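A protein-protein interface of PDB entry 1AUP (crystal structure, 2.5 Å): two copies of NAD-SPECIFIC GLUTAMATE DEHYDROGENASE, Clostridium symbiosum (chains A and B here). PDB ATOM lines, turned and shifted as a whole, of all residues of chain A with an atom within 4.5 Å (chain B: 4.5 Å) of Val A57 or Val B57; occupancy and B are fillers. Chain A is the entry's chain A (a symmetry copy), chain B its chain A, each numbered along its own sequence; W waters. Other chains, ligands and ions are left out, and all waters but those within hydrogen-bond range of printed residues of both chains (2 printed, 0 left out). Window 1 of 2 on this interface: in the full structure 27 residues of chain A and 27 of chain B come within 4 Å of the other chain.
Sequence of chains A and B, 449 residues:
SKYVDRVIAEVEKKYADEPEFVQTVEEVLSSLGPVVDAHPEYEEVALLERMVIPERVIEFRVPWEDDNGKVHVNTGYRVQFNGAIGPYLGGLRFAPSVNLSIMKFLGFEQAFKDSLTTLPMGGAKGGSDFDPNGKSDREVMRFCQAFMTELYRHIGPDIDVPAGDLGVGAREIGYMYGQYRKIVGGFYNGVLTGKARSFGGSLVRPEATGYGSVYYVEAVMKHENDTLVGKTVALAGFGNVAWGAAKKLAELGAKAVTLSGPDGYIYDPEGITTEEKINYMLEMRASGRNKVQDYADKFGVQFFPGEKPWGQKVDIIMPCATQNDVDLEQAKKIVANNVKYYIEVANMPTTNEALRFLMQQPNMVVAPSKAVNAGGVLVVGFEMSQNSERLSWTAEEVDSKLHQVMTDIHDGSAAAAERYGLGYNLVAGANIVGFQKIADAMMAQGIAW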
ATOM      1  N   PRO A  54      -4.066   9.272 -25.150  1.00  0.00           N
ATOM      2  CA  PRO A  54      -4.315  10.400 -24.263  1.00  0.00           C
ATOM      3  C   PRO A  54      -3.118  11.298 -24.361  1.00  0.00           C
ATOM      4  O   PRO A  54      -2.008  10.814 -24.521  1.00  0.00           O
ATOM      5  CB  PRO A  54      -4.373   9.772 -22.865  1.00  0.00           C
ATOM      6  CG  PRO A  54      -4.143   8.281 -23.059  1.00  0.00           C
ATOM      7  CD  PRO A  54      -4.170   7.961 -24.494  1.00  0.00           C
ATOM      8  N   ARG A  56      -1.835  13.043 -21.972  1.00  0.00           N
ATOM      9  CA  ARG A  56      -1.019  12.778 -20.800  1.00  0.00           C
ATOM     10  C   ARG A  56      -1.737  11.888 -19.769  1.00  0.00           C
ATOM     11  O   ARG A  56      -2.929  12.083 -19.483  1.00  0.00           O
ATOM     12  CB  ARG A  56      -0.654  14.120 -20.161  1.00  0.00           C
ATOM     13  CG  ARG A  56      -0.019  14.011 -18.828  1.00  0.00           C
ATOM     14  CD  ARG A  56       0.158  15.388 -18.213  1.00  0.00           C
ATOM     15  NE  ARG A  56       0.859  16.298 -19.101  1.00  0.00           N
ATOM     16  CZ  ARG A  56       0.309  17.373 -19.656  1.00  0.00           C
ATOM     17  NH1 ARG A  56      -0.966  17.676 -19.425  1.00  0.00           N
ATOM     18  NH2 ARG A  56       1.032  18.144 -20.452  1.00  0.00           N
ATOM     19  N   VAL A  57      -1.000  10.934 -19.197  1.00  0.00           N
ATOM     20  CA  VAL A  57      -1.551  10.042 -18.171  1.00  0.00           C
ATOM     21  C   VAL A  57      -0.763  10.089 -16.855  1.00  0.00           C
ATOM     22  O   VAL A  57       0.456   9.970 -16.836  1.00  0.00           O
ATOM     23  CB  VAL A  57      -1.591   8.597 -18.617  1.00  0.00           C
ATOM     24  CG1 VAL A  57      -1.818   7.677 -17.404  1.00  0.00           C
ATOM     25  CG2 VAL A  57      -2.663   8.392 -19.636  1.00  0.00           C
ATOM     26  N   ILE A  58      -1.485  10.190 -15.755  1.00  0.00           N
ATOM     27  CA  ILE A  58      -0.860  10.216 -14.449  1.00  0.00           C
ATOM     28  C   ILE A  58      -1.413   9.167 -13.466  1.00  0.00           C
ATOM     29  O   ILE A  58      -2.632   9.098 -13.195  1.00  0.00           O
ATOM     30  CB  ILE A  58      -0.899  11.610 -13.842  1.00  0.00           C
ATOM     31  CG1 ILE A  58      -0.276  12.616 -14.808  1.00  0.00           C
ATOM     32  CG2 ILE A  58      -0.179  11.630 -12.519  1.00  0.00           C
ATOM     33  CD1 ILE A  58      -1.286  13.574 -15.409  1.00  0.00           C
ATOM     34  N   GLU A  59      -0.508   8.334 -12.971  1.00  0.00           N
ATOM     35  CA  GLU A  59      -0.834   7.321 -11.994  1.00  0.00           C
ATOM     36  C   GLU A  59      -0.008   7.654 -10.796  1.00  0.00           C
ATOM     37  O   GLU A  59       1.129   8.082 -10.922  1.00  0.00           O
ATOM     38  CB  GLU A  59      -0.432   5.956 -12.500  1.00  0.00           C
ATOM     39  CG  GLU A  59      -0.965   5.640 -13.860  1.00  0.00           C
ATOM     40  CD  GLU A  59      -1.196   4.170 -14.035  1.00  0.00           C
ATOM     41  OE1 GLU A  59      -1.019   3.410 -13.055  1.00  0.00           O
ATOM     42  OE2 GLU A  59      -1.527   3.758 -15.159  1.00  0.00           O
ATOM     43  N   ARG A  78      -5.170  10.220 -13.250  1.00  0.00           N
ATOM     44  CA  ARG A  78      -5.708  11.379 -13.920  1.00  0.00           C
ATOM     45  C   ARG A  78      -5.341  11.286 -15.356  1.00  0.00           C
ATOM     46  O   ARG A  78      -4.171  11.338 -15.699  1.00  0.00           O
ATOM     47  CB  ARG A  78      -5.267  12.697 -13.345  1.00  0.00           C
ATOM     48  CG  ARG A  78      -5.993  13.853 -14.035  1.00  0.00           C
ATOM     49  CD  ARG A  78      -7.529  13.641 -13.956  1.00  0.00           C
ATOM     50  NE  ARG A  78      -8.270  14.851 -14.286  1.00  0.00           N
ATOM     51  CZ  ARG A  78      -9.570  15.012 -14.075  1.00  0.00           C
ATOM     52  NH1 ARG A  78     -10.288  14.046 -13.516  1.00  0.00           N
ATOM     53  NH2 ARG A  78     -10.155  16.130 -14.423  1.00  0.00           N
ATOM     54  N   VAL A  79      -6.341  11.080 -16.194  1.00  0.00           N
ATOM     55  CA  VAL A  79      -6.117  10.940 -17.616  1.00  0.00           C
ATOM     56  C   VAL A  79      -6.572  12.174 -18.362  1.00  0.00           C
ATOM     57  O   VAL A  79      -7.762  12.415 -18.521  1.00  0.00           O
ATOM     58  CB  VAL A  79      -6.802   9.684 -18.150  1.00  0.00           C
ATOM     59  CG1 VAL A  79      -6.605   9.541 -19.649  1.00  0.00           C
ATOM     60  CG2 VAL A  79      -6.246   8.466 -17.429  1.00  0.00           C
ATOM     61  N   LEU A 100      -6.602   1.679 -15.386  1.00  0.00           N
ATOM     62  CA  LEU A 100      -6.280   2.544 -16.506  1.00  0.00           C
ATOM     63  C   LEU A 100      -7.213   2.360 -17.660  1.00  0.00           C
ATOM     64  O   LEU A 100      -7.606   3.316 -18.311  1.00  0.00           O
ATOM     65  CB  LEU A 100      -4.822   2.354 -16.954  1.00  0.00           C
ATOM     66  CG  LEU A 100      -4.289   3.392 -17.977  1.00  0.00           C
ATOM     67  CD1 LEU A 100      -4.292   4.802 -17.380  1.00  0.00           C
ATOM     68  CD2 LEU A 100      -2.886   3.061 -18.443  1.00  0.00           C
ATOM     69  N   PRO B  54       4.936   2.698  -7.826  1.00  0.00           N
ATOM     70  CA  PRO B  54       5.778   3.838  -8.160  1.00  0.00           C
ATOM     71  C   PRO B  54       5.131   5.045  -7.549  1.00  0.00           C
ATOM     72  O   PRO B  54       3.913   5.116  -7.489  1.00  0.00           O
ATOM     73  CB  PRO B  54       5.696   3.929  -9.689  1.00  0.00           C
ATOM     74  CG  PRO B  54       4.781   2.799 -10.133  1.00  0.00           C
ATOM     75  CD  PRO B  54       4.494   1.918  -8.990  1.00  0.00           C
ATOM     76  N   ARG B  56       5.082   8.021  -8.787  1.00  0.00           N
ATOM     77  CA  ARG B  56       4.375   8.701  -9.859  1.00  0.00           C
ATOM     78  C   ARG B  56       4.709   8.126 -11.246  1.00  0.00           C
ATOM     79  O   ARG B  56       5.880   7.848 -11.553  1.00  0.00           O
ATOM     80  CB  ARG B  56       4.748  10.185  -9.808  1.00  0.00           C
ATOM     81  CG  ARG B  56       4.290  10.972 -10.976  1.00  0.00           C
ATOM     82  CD  ARG B  56       4.842  12.384 -10.912  1.00  0.00           C
ATOM     83  NE  ARG B  56       4.548  13.029  -9.644  1.00  0.00           N
ATOM     84  CZ  ARG B  56       5.467  13.366  -8.745  1.00  0.00           C
ATOM     85  NH1 ARG B  56       6.754  13.110  -8.966  1.00  0.00           N
ATOM     86  NH2 ARG B  56       5.099  13.953  -7.618  1.00  0.00           N
ATOM     87  N   VAL B  57       3.684   7.976 -12.087  1.00  0.00           N
ATOM     88  CA  VAL B  57       3.871   7.475 -13.453  1.00  0.00           C
ATOM     89  C   VAL B  57       3.349   8.445 -14.521  1.00  0.00           C
ATOM     90  O   VAL B  57       2.224   8.926 -14.452  1.00  0.00           O
ATOM     91  CB  VAL B  57       3.186   6.145 -13.683  1.00  0.00           C
ATOM     92  CG1 VAL B  57       3.096   5.853 -15.191  1.00  0.00           C
ATOM     93  CG2 VAL B  57       3.918   5.050 -12.980  1.00  0.00           C
ATOM     94  N   ILE B  58       4.154   8.664 -15.543  1.00  0.00           N
ATOM     95  CA  ILE B  58       3.764   9.538 -16.629  1.00  0.00           C
ATOM     96  C   ILE B  58       3.875   8.896 -18.025  1.00  0.00           C
ATOM     97  O   ILE B  58       4.946   8.394 -18.435  1.00  0.00           O
ATOM     98  CB  ILE B  58       4.514  10.861 -16.574  1.00  0.00           C
ATOM     99  CG1 ILE B  58       4.324  11.510 -15.205  1.00  0.00           C
ATOM    100  CG2 ILE B  58       4.040  11.782 -17.669  1.00  0.00           C
ATOM    101  CD1 ILE B  58       5.587  11.523 -14.367  1.00  0.00           C
ATOM    102  N   GLU B  59       2.750   8.885 -18.725  1.00  0.00           N
ATOM    103  CA  GLU B  59       2.677   8.372 -20.074  1.00  0.00           C
ATOM    104  C   GLU B  59       2.242   9.531 -20.909  1.00  0.00           C
ATOM    105  O   GLU B  59       1.425  10.334 -20.482  1.00  0.00           O
ATOM    106  CB  GLU B  59       1.634   7.284 -20.166  1.00  0.00           C
ATOM    107  CG  GLU B  59       1.802   6.205 -19.147  1.00  0.00           C
ATOM    108  CD  GLU B  59       1.304   4.885 -19.651  1.00  0.00           C
ATOM    109  OE1 GLU B  59       0.907   4.802 -20.836  1.00  0.00           O
ATOM    110  OE2 GLU B  59       1.277   3.927 -18.861  1.00  0.00           O
ATOM    111  N   ARG B  78       7.690   8.062 -18.187  1.00  0.00           N
ATOM    112  CA  ARG B  78       8.624   8.420 -17.147  1.00  0.00           C
ATOM    113  C   ARG B  78       8.097   7.898 -15.862  1.00  0.00           C
ATOM    114  O   ARG B  78       7.053   8.331 -15.400  1.00  0.00           O
ATOM    115  CB  ARG B  78       8.912   9.892 -17.043  1.00  0.00           C
ATOM    116  CG  ARG B  78      10.008  10.151 -16.008  1.00  0.00           C
ATOM    117  CD  ARG B  78      11.269   9.309 -16.344  1.00  0.00           C
ATOM    118  NE  ARG B  78      12.443   9.759 -15.610  1.00  0.00           N
ATOM    119  CZ  ARG B  78      13.685   9.372 -15.875  1.00  0.00           C
ATOM    120  NH1 ARG B  78      13.931   8.534 -16.874  1.00  0.00           N
ATOM    121  NH2 ARG B  78      14.679   9.816 -15.146  1.00  0.00           N
ATOM    122  N   VAL B  79       8.785   6.912 -15.314  1.00  0.00           N
ATOM    123  CA  VAL B  79       8.363   6.293 -14.077  1.00  0.00           C
ATOM    124  C   VAL B  79       9.251   6.713 -12.928  1.00  0.00           C
ATOM    125  O   VAL B  79      10.389   6.280 -12.815  1.00  0.00           O
ATOM    126  CB  VAL B  79       8.323   4.773 -14.220  1.00  0.00           C
ATOM    127  CG1 VAL B  79       7.913   4.105 -12.918  1.00  0.00           C
ATOM    128  CG2 VAL B  79       7.350   4.400 -15.328  1.00  0.00           C
ATOM    129  N   LEU B 100       4.748  -0.132 -20.129  1.00  0.00           N
ATOM    130  CA  LEU B 100       4.739   0.203 -18.718  1.00  0.00           C
ATOM    131  C   LEU B 100       5.344  -0.871 -17.869  1.00  0.00           C
ATOM    132  O   LEU B 100       6.058  -0.595 -16.918  1.00  0.00           O
ATOM    133  CB  LEU B 100       3.320   0.538 -18.233  1.00  0.00           C
ATOM    134  CG  LEU B 100       3.216   1.146 -16.810  1.00  0.00           C
ATOM    135  CD1 LEU B 100       3.940   2.493 -16.734  1.00  0.00           C
ATOM    136  CD2 LEU B 100       1.777   1.338 -16.377  1.00  0.00           C
HETATM  137  O   HOH W   1       1.521   5.023  -9.887  1.00  0.00           O
HETATM  138  O   HOH W   2      -0.220   8.597 -22.686  1.00  0.00           O
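Printed residues of chain B that touch a printed residue of chain A: Arg B56, Val B57, Ile B58 and Glu B59.
Hydrophobic or aromatic side chains of chain B that line the printed part of chain A: Val B57.
Among the printed residues, 7 pairs touch across the chains.
The backbone carbonyl oxygen (O) of Ile B58 is in hydrogen-bond range of the backbone NH (N) of Arg B78, at 2.8 Å.
O of Ile A58 sits at hydrogen-bond distance from N of Arg A78.
N of Val B57 is in hydrogen-bond range of O of Glu A59 (2.8 Å).
The backbone NH (N) of Val A57 is in hydrogen-bond range of the backbone carbonyl oxygen (O) of Glu B59, 2.8 Å away.
The backbone carbonyl oxygen of Val A57 lies close to the backbone carbonyl oxygen of Val B57 (3.1 Å).
Of the printed residues of chain B, Ile A58 touches Val B57.
Printed residues of chain B within 4 Å of Glu A59: Arg B56 and Val B57.
Leu A100 touches none of the printed residues of chain B.
Val B57 touches just these residues of chain A: Val A57 (3.1 Å), Ile A58 (3.3 Å) and Glu A59 (2.8 Å).
Of the printed residues of chain A, Ile B58 touches Val A57.
Of the printed residues of chain A, Glu B59 touches Arg A56 (3.5 Å) and Val A57 (2.8 Å).
The nearest printed residue of chain A that does not touch Val B57 is Arg A78 (6.9 Å).
Among the printed residues, pairs that only touch across the chains: Val A57 with Ile B58, Ile A58 with Val B57, Arg A56 with Glu B59 and Glu A59 with Arg B56.
Water W2 lies within hydrogen-bond range of the backbone carbonyl oxygen of Glu B59 and the backbone carbonyl oxygen of Pro A54.
Water W1 lies within hydrogen-bond range of O of Glu A59 (3.3 Å) and O of Pro B54 (3.4 Å).
Arg A56 touches Glu B59, and with the chains exchanged Glu A59 touches Arg B56.
Val A57 touches its own counterpart, Val B57.
Val A57 touches Ile B58, and with the chains exchanged Ile A58 touches Val B57.
Val A57 touches Glu B59, and with the chains exchanged Glu A59 touches Val B57.
Positions printed for both chains: 54, 56, 57, 58, 59, 78, 79 and 100.
Of the 7 pairs that touch across the chains among the printed residues, 7 have their exchanged pair printed and touching as well.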
